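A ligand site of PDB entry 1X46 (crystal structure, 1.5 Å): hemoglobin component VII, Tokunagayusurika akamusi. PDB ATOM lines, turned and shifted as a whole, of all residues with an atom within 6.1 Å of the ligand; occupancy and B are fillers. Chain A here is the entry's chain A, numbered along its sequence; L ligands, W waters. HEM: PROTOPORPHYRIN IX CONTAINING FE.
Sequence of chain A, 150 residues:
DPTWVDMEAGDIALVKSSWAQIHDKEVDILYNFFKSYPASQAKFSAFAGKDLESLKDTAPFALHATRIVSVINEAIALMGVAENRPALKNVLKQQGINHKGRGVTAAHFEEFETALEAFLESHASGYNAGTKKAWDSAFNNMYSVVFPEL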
ATOM      1  N   PHE A  33      22.811 -15.702 -15.334  1.00  0.00           N
ATOM      2  CA  PHE A  33      24.205 -15.537 -14.939  1.00  0.00           C
ATOM      3  C   PHE A  33      25.051 -16.678 -15.470  1.00  0.00           C
ATOM      4  O   PHE A  33      26.065 -16.401 -16.127  1.00  0.00           O
ATOM      5  CB  PHE A  33      24.288 -15.424 -13.388  1.00  0.00           C
ATOM      6  CG  PHE A  33      25.701 -15.375 -12.854  1.00  0.00           C
ATOM      7  CD1 PHE A  33      26.652 -14.517 -13.409  1.00  0.00           C
ATOM      8  CD2 PHE A  33      26.092 -16.216 -11.794  1.00  0.00           C
ATOM      9  CE1 PHE A  33      27.968 -14.477 -12.912  1.00  0.00           C
ATOM     10  CE2 PHE A  33      27.403 -16.188 -11.293  1.00  0.00           C
ATOM     11  CZ  PHE A  33      28.337 -15.299 -11.847  1.00  0.00           C
ATOM     12  N   SER A  40      31.799 -19.346 -14.577  1.00  0.00           N
ATOM     13  CA  SER A  40      31.399 -19.176 -13.176  1.00  0.00           C
ATOM     14  C   SER A  40      30.688 -20.404 -12.618  1.00  0.00           C
ATOM     15  O   SER A  40      30.901 -20.797 -11.481  1.00  0.00           O
ATOM     16  CB  SER A  40      30.517 -17.961 -13.069  1.00  0.00           C
ATOM     17  OG  SER A  40      31.295 -16.863 -13.476  1.00  0.00           O
ATOM     18  N   LYS A  43      32.656 -23.206 -10.927  1.00  0.00           N
ATOM     19  CA  LYS A  43      33.148 -23.055  -9.545  1.00  0.00           C
ATOM     20  C   LYS A  43      32.246 -23.712  -8.499  1.00  0.00           C
ATOM     21  O   LYS A  43      32.664 -23.909  -7.333  1.00  0.00           O
ATOM     22  CB  LYS A  43      33.326 -21.581  -9.222  1.00  0.00           C
ATOM     23  CG  LYS A  43      34.233 -20.858 -10.189  1.00  0.00           C
ATOM     24  CD  LYS A  43      34.680 -19.526  -9.646  1.00  0.00           C
ATOM     25  CE  LYS A  43      35.566 -18.803 -10.639  1.00  0.00           C
ATOM     26  NZ  LYS A  43      36.958 -19.266 -10.476  1.00  0.00           N
ATOM     27  N   PHE A  44      31.017 -24.017  -8.885  1.00  0.00           N
ATOM     28  CA  PHE A  44      30.017 -24.497  -7.917  1.00  0.00           C
ATOM     29  C   PHE A  44      30.007 -25.991  -7.725  1.00  0.00           C
ATOM     30  O   PHE A  44      29.893 -26.732  -8.687  1.00  0.00           O
ATOM     31  CB  PHE A  44      28.620 -24.044  -8.309  1.00  0.00           C
ATOM     32  CG  PHE A  44      28.396 -22.559  -8.177  1.00  0.00           C
ATOM     33  CD1 PHE A  44      27.635 -22.042  -7.120  1.00  0.00           C
ATOM     34  CD2 PHE A  44      28.995 -21.685  -9.076  1.00  0.00           C
ATOM     35  CE1 PHE A  44      27.452 -20.680  -6.998  1.00  0.00           C
ATOM     36  CE2 PHE A  44      28.802 -20.321  -8.935  1.00  0.00           C
ATOM     37  CZ  PHE A  44      28.038 -19.827  -7.902  1.00  0.00           C
ATOM     38  N   SER A  45      30.057 -26.459  -6.482  1.00  0.00           N
ATOM     39  CA  SER A  45      30.047 -27.889  -6.204  1.00  0.00           C
ATOM     40  C   SER A  45      28.813 -28.598  -6.739  1.00  0.00           C
ATOM     41  O   SER A  45      28.906 -29.717  -7.252  1.00  0.00           O
ATOM     42  CB  SER A  45      30.186 -28.175  -4.701  1.00  0.00           C
ATOM     43  OG  SER A  45      31.388 -27.598  -4.214  1.00  0.00           O
ATOM     44  N   ALA A  46      27.653 -27.947  -6.650  1.00  0.00           N
ATOM     45  CA  ALA A  46      26.423 -28.561  -7.096  1.00  0.00           C
ATOM     46  C   ALA A  46      26.208 -28.466  -8.609  1.00  0.00           C
ATOM     47  O   ALA A  46      25.394 -29.199  -9.143  1.00  0.00           O
ATOM     48  CB  ALA A  46      25.193 -27.957  -6.377  1.00  0.00           C
ATOM     49  N   HIS A  64      20.211 -22.596  -4.543  1.00  0.00           N
ATOM     50  CA  HIS A  64      21.287 -21.622  -4.607  1.00  0.00           C
ATOM     51  C   HIS A  64      20.753 -20.234  -5.085  1.00  0.00           C
ATOM     52  O   HIS A  64      21.175 -19.191  -4.571  1.00  0.00           O
ATOM     53  CB  HIS A  64      22.452 -22.043  -5.504  1.00  0.00           C
ATOM     54  CG  HIS A  64      23.579 -21.115  -5.358  1.00  0.00           C
ATOM     55  ND1 HIS A  64      24.293 -21.034  -4.176  1.00  0.00           N
ATOM     56  CD2 HIS A  64      23.982 -20.065  -6.111  1.00  0.00           C
ATOM     57  CE1 HIS A  64      25.150 -20.037  -4.253  1.00  0.00           C
ATOM     58  NE2 HIS A  64      24.960 -19.407  -5.395  1.00  0.00           N
ATOM     59  N   ARG A  67      19.281 -18.572  -2.166  1.00  0.00           N
ATOM     60  CA  ARG A  67      20.320 -18.083  -1.256  1.00  0.00           C
ATOM     61  C   ARG A  67      20.900 -16.750  -1.730  1.00  0.00           C
ATOM     62  O   ARG A  67      21.076 -15.837  -0.910  1.00  0.00           O
ATOM     63  CB  ARG A  67      21.439 -19.126  -1.127  1.00  0.00           C
ATOM     64  CG  ARG A  67      21.001 -20.326  -0.318  1.00  0.00           C
ATOM     65  CD  ARG A  67      22.062 -21.434  -0.274  1.00  0.00           C
ATOM     66  NE  ARG A  67      21.720 -22.415   0.753  1.00  0.00           N
ATOM     67  CZ  ARG A  67      22.057 -23.684   0.761  1.00  0.00           C
ATOM     68  NH1 ARG A  67      22.809 -24.210  -0.218  1.00  0.00           N
ATOM     69  NH2 ARG A  67      21.631 -24.442   1.787  1.00  0.00           N
ATOM     70  N   ILE A  68      21.224 -16.606  -3.031  1.00  0.00           N
ATOM     71  CA  ILE A  68      21.817 -15.379  -3.563  1.00  0.00           C
ATOM     72  C   ILE A  68      20.819 -14.250  -3.375  1.00  0.00           C
ATOM     73  O   ILE A  68      21.166 -13.179  -2.883  1.00  0.00           O
ATOM     74  CB  ILE A  68      22.130 -15.505  -5.086  1.00  0.00           C
ATOM     75  CG1 ILE A  68      23.287 -16.471  -5.300  1.00  0.00           C
ATOM     76  CG2 ILE A  68      22.499 -14.102  -5.699  1.00  0.00           C
ATOM     77  CD1 ILE A  68      23.535 -16.783  -6.787  1.00  0.00           C
ATOM     78  N   VAL A  69      19.586 -14.513  -3.760  1.00  0.00           N
ATOM     79  CA  VAL A  69      18.572 -13.463  -3.761  1.00  0.00           C
ATOM     80  C   VAL A  69      18.194 -13.028  -2.354  1.00  0.00           C
ATOM     81  O   VAL A  69      17.918 -11.865  -2.107  1.00  0.00           O
ATOM     82  CB  VAL A  69      17.331 -13.915  -4.581  1.00  0.00           C
ATOM     83  CG1 VAL A  69      16.082 -13.064  -4.235  1.00  0.00           C
ATOM     84  CG2 VAL A  69      17.669 -13.814  -6.051  1.00  0.00           C
ATOM     85  N   VAL A  71      20.257 -12.671   0.091  1.00  0.00           N
ATOM     86  CA  VAL A  71      21.253 -11.684   0.501  1.00  0.00           C
ATOM     87  C   VAL A  71      21.034 -10.380  -0.249  1.00  0.00           C
ATOM     88  O   VAL A  71      21.075  -9.298   0.344  1.00  0.00           O
ATOM     89  CB  VAL A  71      22.664 -12.222   0.240  1.00  0.00           C
ATOM     90  CG1 VAL A  71      23.732 -11.130   0.488  1.00  0.00           C
ATOM     91  CG2 VAL A  71      22.939 -13.413   1.117  1.00  0.00           C
ATOM     92  N   ILE A  72      20.788 -10.441  -1.545  1.00  0.00           N
ATOM     93  CA  ILE A  72      20.528  -9.196  -2.281  1.00  0.00           C
ATOM     94  C   ILE A  72      19.316  -8.466  -1.725  1.00  0.00           C
ATOM     95  O   ILE A  72      19.362  -7.250  -1.545  1.00  0.00           O
ATOM     96  CB  ILE A  72      20.384  -9.454  -3.814  1.00  0.00           C
ATOM     97  CG1 ILE A  72      21.664 -10.065  -4.369  1.00  0.00           C
ATOM     98  CG2 ILE A  72      20.080  -8.128  -4.570  1.00  0.00           C
ATOM     99  CD1 ILE A  72      21.621 -10.476  -5.863  1.00  0.00           C
ATOM    100  N   GLN A  95      30.090 -11.201   2.694  1.00  0.00           N
ATOM    101  CA  GLN A  95      30.033 -11.834   1.365  1.00  0.00           C
ATOM    102  C   GLN A  95      31.383 -11.798   0.685  1.00  0.00           C
ATOM    103  O   GLN A  95      31.780 -12.768   0.044  1.00  0.00           O
ATOM    104  CB  GLN A  95      28.951 -11.207   0.468  1.00  0.00           C
ATOM    105  CG  GLN A  95      27.507 -11.456   0.972  1.00  0.00           C
ATOM    106  CD  GLN A  95      27.197 -12.927   1.088  1.00  0.00           C
ATOM    107  OE1 GLN A  95      27.493 -13.696   0.168  1.00  0.00           O
ATOM    108  NE2 GLN A  95      26.666 -13.346   2.230  1.00  0.00           N
ATOM    109  N   ASN A  98      33.512 -14.451   2.470  1.00  0.00           N
ATOM    110  CA  ASN A  98      33.087 -15.793   2.096  1.00  0.00           C
ATOM    111  C   ASN A  98      33.541 -16.149   0.681  1.00  0.00           C
ATOM    112  O   ASN A  98      33.953 -17.278   0.407  1.00  0.00           O
ATOM    113  CB  ASN A  98      31.576 -15.956   2.198  1.00  0.00           C
ATOM    114  CG  ASN A  98      31.035 -15.816   3.614  1.00  0.00           C
ATOM    115  OD1 ASN A  98      31.800 -15.796   4.593  1.00  0.00           O
ATOM    116  ND2 ASN A  98      29.730 -15.701   3.726  1.00  0.00           N
ATOM    117  N   HIS A  99      33.451 -15.186  -0.234  1.00  0.00           N
ATOM    118  CA  HIS A  99      33.805 -15.455  -1.603  1.00  0.00           C
ATOM    119  C   HIS A  99      35.306 -15.480  -1.858  1.00  0.00           C
ATOM    120  O   HIS A  99      35.756 -16.110  -2.802  1.00  0.00           O
ATOM    121  CB  HIS A  99      33.068 -14.499  -2.557  1.00  0.00           C
ATOM    122  CG  HIS A  99      31.621 -14.858  -2.727  1.00  0.00           C
ATOM    123  ND1 HIS A  99      30.630 -14.394  -1.881  1.00  0.00           N
ATOM    124  CD2 HIS A  99      31.010 -15.682  -3.605  1.00  0.00           C
ATOM    125  CE1 HIS A  99      29.471 -14.906  -2.255  1.00  0.00           C
ATOM    126  NE2 HIS A  99      29.671 -15.684  -3.299  1.00  0.00           N
ATOM    127  N   ARG A 102      36.532 -18.881  -1.962  1.00  0.00           N
ATOM    128  CA  ARG A 102      36.062 -19.638  -3.123  1.00  0.00           C
ATOM    129  C   ARG A 102      36.789 -19.258  -4.408  1.00  0.00           C
ATOM    130  O   ARG A 102      36.421 -19.731  -5.469  1.00  0.00           O
ATOM    131  CB  ARG A 102      34.568 -19.389  -3.319  1.00  0.00           C
ATOM    132  CG  ARG A 102      33.732 -19.818  -2.083  1.00  0.00           C
ATOM    133  CD  ARG A 102      32.336 -19.268  -2.079  1.00  0.00           C
ATOM    134  NE  ARG A 102      31.657 -19.597  -0.844  1.00  0.00           N
ATOM    135  CZ  ARG A 102      30.759 -18.843  -0.222  1.00  0.00           C
ATOM    136  NH1 ARG A 102      30.357 -17.690  -0.748  1.00  0.00           N
ATOM    137  NH2 ARG A 102      30.263 -19.250   0.946  1.00  0.00           N
ATOM    138  N   VAL A 104      36.818 -16.346  -5.924  1.00  0.00           N
ATOM    139  CA  VAL A 104      36.020 -15.445  -6.764  1.00  0.00           C
ATOM    140  C   VAL A 104      36.716 -14.085  -6.823  1.00  0.00           C
ATOM    141  O   VAL A 104      37.088 -13.536  -5.766  1.00  0.00           O
ATOM    142  CB  VAL A 104      34.582 -15.326  -6.188  1.00  0.00           C
ATOM    143  CG1 VAL A 104      33.768 -14.306  -6.978  1.00  0.00           C
ATOM    144  CG2 VAL A 104      33.894 -16.688  -6.210  1.00  0.00           C
ATOM    145  N   THR A 105      36.888 -13.562  -8.033  1.00  0.00           N
ATOM    146  CA  THR A 105      37.621 -12.308  -8.259  1.00  0.00           C
ATOM    147  C   THR A 105      36.702 -11.100  -8.362  1.00  0.00           C
ATOM    148  O   THR A 105      35.450 -11.223  -8.495  1.00  0.00           O
ATOM    149  CB  THR A 105      38.421 -12.348  -9.589  1.00  0.00           C
ATOM    150  OG1 THR A 105      37.501 -12.487 -10.684  1.00  0.00           O
ATOM    151  CG2 THR A 105      39.302 -13.610  -9.714  1.00  0.00           C
ATOM    152  N   HIS A 108      34.882 -11.347 -11.542  1.00  0.00           N
ATOM    153  CA  HIS A 108      33.717 -12.240 -11.414  1.00  0.00           C
ATOM    154  C   HIS A 108      32.507 -11.495 -10.900  1.00  0.00           C
ATOM    155  O   HIS A 108      31.392 -11.718 -11.383  1.00  0.00           O
ATOM    156  CB  HIS A 108      33.953 -13.430 -10.486  1.00  0.00           C
ATOM    157  CG  HIS A 108      34.964 -14.389 -10.982  1.00  0.00           C
ATOM    158  ND1 HIS A 108      35.156 -14.613 -12.334  1.00  0.00           N
ATOM    159  CD2 HIS A 108      35.794 -15.199 -10.322  1.00  0.00           C
ATOM    160  CE1 HIS A 108      36.143 -15.481 -12.477  1.00  0.00           C
ATOM    161  NE2 HIS A 108      36.527 -15.874 -11.273  1.00  0.00           N
ATOM    162  N   PHE A 109      32.691 -10.639  -9.900  1.00  0.00           N
ATOM    163  CA  PHE A 109      31.564  -9.812  -9.427  1.00  0.00           C
ATOM    164  C   PHE A 109      31.054  -8.869 -10.507  1.00  0.00           C
ATOM    165  O   PHE A 109      29.851  -8.713 -10.699  1.00  0.00           O
ATOM    166  CB  PHE A 109      31.900  -9.092  -8.116  1.00  0.00           C
ATOM    167  CG  PHE A 109      31.736  -9.973  -6.893  1.00  0.00           C
ATOM    168  CD1 PHE A 109      30.470 -10.241  -6.386  1.00  0.00           C
ATOM    169  CD2 PHE A 109      32.851 -10.539  -6.272  1.00  0.00           C
ATOM    170  CE1 PHE A 109      30.304 -11.064  -5.289  1.00  0.00           C
ATOM    171  CE2 PHE A 109      32.697 -11.358  -5.154  1.00  0.00           C
ATOM    172  CZ  PHE A 109      31.445 -11.634  -4.655  1.00  0.00           C
ATOM    173  N   PHE A 112      28.854 -10.756 -12.815  1.00  0.00           N
ATOM    174  CA  PHE A 112      27.509 -10.935 -12.236  1.00  0.00           C
ATOM    175  C   PHE A 112      26.699  -9.650 -12.453  1.00  0.00           C
ATOM    176  O   PHE A 112      25.530  -9.698 -12.839  1.00  0.00           O
ATOM    177  CB  PHE A 112      27.616 -11.284 -10.739  1.00  0.00           C
ATOM    178  CG  PHE A 112      26.268 -11.524 -10.112  1.00  0.00           C
ATOM    179  CD1 PHE A 112      25.782 -12.823 -10.036  1.00  0.00           C
ATOM    180  CD2 PHE A 112      25.479 -10.462  -9.650  1.00  0.00           C
ATOM    181  CE1 PHE A 112      24.519 -13.066  -9.482  1.00  0.00           C
ATOM    182  CE2 PHE A 112      24.216 -10.696  -9.092  1.00  0.00           C
ATOM    183  CZ  PHE A 112      23.748 -12.018  -9.039  1.00  0.00           C
ATOM    184  N   PHE A 139      26.358  -0.746  -7.254  1.00  0.00           N
ATOM    185  CA  PHE A 139      27.471  -1.678  -7.419  1.00  0.00           C
ATOM    186  C   PHE A 139      28.836  -1.074  -7.055  1.00  0.00           C
ATOM    187  O   PHE A 139      29.646  -1.740  -6.438  1.00  0.00           O
ATOM    188  CB  PHE A 139      27.503  -2.292  -8.822  1.00  0.00           C
ATOM    189  CG  PHE A 139      26.590  -3.485  -8.966  1.00  0.00           C
ATOM    190  CD1 PHE A 139      26.959  -4.697  -8.397  1.00  0.00           C
ATOM    191  CD2 PHE A 139      25.402  -3.415  -9.663  1.00  0.00           C
ATOM    192  CE1 PHE A 139      26.121  -5.844  -8.515  1.00  0.00           C
ATOM    193  CE2 PHE A 139      24.591  -4.550  -9.783  1.00  0.00           C
ATOM    194  CZ  PHE A 139      24.959  -5.743  -9.208  1.00  0.00           C
ATOM    195  N   MET A 142      28.950  -1.266  -3.335  1.00  0.00           N
ATOM    196  CA  MET A 142      29.184  -2.659  -2.943  1.00  0.00           C
ATOM    197  C   MET A 142      30.663  -3.043  -3.128  1.00  0.00           C
ATOM    198  O   MET A 142      31.301  -3.609  -2.219  1.00  0.00           O
ATOM    199  CB  MET A 142      28.297  -3.611  -3.779  1.00  0.00           C
ATOM    200  CG  MET A 142      28.658  -5.076  -3.647  1.00  0.00           C
ATOM    201  SD  MET A 142      27.762  -6.031  -4.959  1.00  0.00           S
ATOM    202  CE  MET A 142      28.810  -7.469  -5.088  1.00  0.00           C
HETATM  203  CHA HEM L   1      28.007 -19.379  -2.453  1.00  0.00           C
HETATM  204  CHB HEM L   1      25.823 -15.052  -2.388  1.00  0.00           C
HETATM  205  CHC HEM L   1      28.266 -13.775  -6.363  1.00  0.00           C
HETATM  206  CHD HEM L   1      30.452 -18.087  -6.470  1.00  0.00           C
HETATM  207  C1A HEM L   1      27.177 -18.348  -2.140  1.00  0.00           C
HETATM  208  C2A HEM L   1      26.203 -18.375  -1.066  1.00  0.00           C
HETATM  209  C3A HEM L   1      25.614 -17.190  -1.063  1.00  0.00           C
HETATM  210  C4A HEM L   1      26.202 -16.347  -2.081  1.00  0.00           C
HETATM  211  CMA HEM L   1      24.500 -16.731  -0.096  1.00  0.00           C
HETATM  212  CAA HEM L   1      25.860 -19.620  -0.191  1.00  0.00           C
HETATM  213  CBA HEM L   1      26.844 -19.945   0.948  1.00  0.00           C
HETATM  214  CGA HEM L   1      26.847 -18.849   1.980  1.00  0.00           C
HETATM  215  O1A HEM L   1      27.917 -18.265   2.243  1.00  0.00           O
HETATM  216  O2A HEM L   1      25.766 -18.557   2.570  1.00  0.00           O
HETATM  217  C1B HEM L   1      26.249 -14.347  -3.472  1.00  0.00           C
HETATM  218  C2B HEM L   1      25.813 -13.026  -3.878  1.00  0.00           C
HETATM  219  C3B HEM L   1      26.499 -12.670  -4.988  1.00  0.00           C
HETATM  220  C4B HEM L   1      27.399 -13.770  -5.285  1.00  0.00           C
HETATM  221  CMB HEM L   1      24.720 -12.217  -3.132  1.00  0.00           C
HETATM  222  CAB HEM L   1      26.457 -11.400  -5.865  1.00  0.00           C
HETATM  223  CBB HEM L   1      25.766 -10.294  -5.572  1.00  0.00           C
HETATM  224  C1C HEM L   1      29.069 -14.809  -6.756  1.00  0.00           C
HETATM  225  C2C HEM L   1      29.963 -14.847  -7.916  1.00  0.00           C
HETATM  226  C3C HEM L   1      30.536 -16.049  -7.960  1.00  0.00           C
HETATM  227  C4C HEM L   1      30.067 -16.810  -6.814  1.00  0.00           C
HETATM  228  CMC HEM L   1      30.186 -13.674  -8.892  1.00  0.00           C
HETATM  229  CAC HEM L   1      31.565 -16.567  -9.002  1.00  0.00           C
HETATM  230  C1D HEM L   1      30.022 -18.786  -5.375  1.00  0.00           C
HETATM  231  C2D HEM L   1      30.472 -20.123  -5.065  1.00  0.00           C
HETATM  232  C3D HEM L   1      29.729 -20.511  -3.817  1.00  0.00           C
HETATM  233  C4D HEM L   1      28.865 -19.383  -3.536  1.00  0.00           C
HETATM  234  CMD HEM L   1      31.508 -20.954  -5.842  1.00  0.00           C
HETATM  235  CAD HEM L   1      29.850 -21.859  -3.070  1.00  0.00           C
HETATM  236  CBD HEM L   1      28.984 -22.930  -3.730  1.00  0.00           C
HETATM  237  CGD HEM L   1      29.208 -24.277  -3.068  1.00  0.00           C
HETATM  238  O1D HEM L   1      29.667 -24.322  -1.905  1.00  0.00           O
HETATM  239  O2D HEM L   1      28.933 -25.307  -3.722  1.00  0.00           O
HETATM  240  NA  HEM L   1      27.154 -17.104  -2.719  1.00  0.00           N
HETATM  241  NB  HEM L   1      27.212 -14.786  -4.387  1.00  0.00           N
HETATM  242  NC  HEM L   1      29.168 -16.020  -6.092  1.00  0.00           N
HETATM  243  ND  HEM L   1      29.088 -18.356  -4.433  1.00  0.00           N
HETATM  244 FE   HEM L   1      28.159 -16.568  -4.403  1.00  0.00          FE
HETATM  245  O   HOH W   1      25.824 -15.985   3.406  1.00  0.00           O
HETATM  246  O   HOH W   2      26.816 -22.920  -0.915  1.00  0.00           O
HETATM  247  O   HOH W   3      26.707 -17.305  -5.698  1.00  0.00           O
HETATM  248  O   HOH W   4      28.623 -18.774   4.819  1.00  0.00           O
HETATM  249  O   HOH W   5      28.586 -16.060   0.878  1.00  0.00           O
HETATM  250  O   HOH W   6      31.964 -24.665  -4.623  1.00  0.00           O
HETATM  251  O   HOH W   7      23.395 -19.703   2.543  1.00  0.00           O
HETATM  252  O   HOH W   8      27.122 -25.385  -5.449  1.00  0.00           O
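Water W8 lies within hydrogen-bond range of an oxygen (O2D) of the ligand (2.5 Å), the backbone NH (N) of Ala 46 (2.9 Å) and the backbone NH (N) of Ser 45 (3.3 Å).
Water W5 lies within hydrogen-bond range of an oxygen (O1A) of the ligand (2.7 Å), the side-chain amide oxygen of Gln 95 (2.7 Å), the guanidinium group of Arg 102 (2.9 Å) and the side-chain amide nitrogen of Asn 98 (3.1 Å).
Water W1 lies within hydrogen-bond range of an oxygen (O2A) of the ligand (2.7 Å) and the side-chain amide nitrogen of Gln 95 (3.0 Å).
Water W4 bridges an oxygen (O1A) of the ligand (2.7 Å) and the side-chain amide nitrogen (ND2) of Asn 98 (3.4 Å).
Water W6 lies within hydrogen-bond range of O of Lys 43 (2.9 Å), OG of Ser 45 (3.0 Å) and O2D of the ligand (3.2 Å).
A ring nitrogen (NE2) of His 99 binds an iron atom (FE) of the ligand, 2.1 Å away.
NH2 of Arg 102 is in salt-bridge range of O1A of the ligand, at 2.9 Å.
N of Ser 45 lies within hydrogen-bond range of O2D of the ligand (3.2 Å).
An oxygen (O2D) of the ligand sits close to the side-chain hydroxyl (OG) of Ser 45.
An oxygen (O1A) of the ligand lies within hydrogen-bond range of the side-chain amide nitrogen (ND2) of Asn 98, 3.5 Å away.
NH1 of Arg 102 sits close to ND1 of His 99 (3.5 Å).
The backbone carbonyl oxygen (O) of Gln 95 sits at hydrogen-bond distance from a ring nitrogen (ND1) of His 99, 2.8 Å away.
O of His 99 lies within hydrogen-bond range of N of Val 104, at 3.3 Å.
The guanidinium group (NE) of Arg 102 lies within hydrogen-bond range of the backbone carbonyl oxygen (O) of Asn 98 (3.5 Å).
The side-chain hydroxyl of Thr 105 sits at hydrogen-bond distance from the backbone NH of His 108 (3.0 Å).
Residues that only touch the ligand: Phe 44 (3.3 Å), Gln 95 (3.3 Å), His 64 (3.4 Å), His 108 (3.4 Å), Lys 43 (3.5 Å), Phe 109 (3.6 Å), Arg 67 (3.6 Å), Val 104 (3.6 Å), Ile 68 (3.7 Å), Phe 33 (3.8 Å), Val 71 (3.9 Å), Phe 112 (3.9 Å) and Ile 72 (3.9 Å).
Within 4 Å of the ligand: Phe 33, Lys 43, Phe 44, Ser 45, His 64, Arg 67, Ile 68, Val 71, Ile 72, Gln 95, Asn 98, His 99, Arg 102, Val 104, His 108, Phe 109 and Phe 112.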
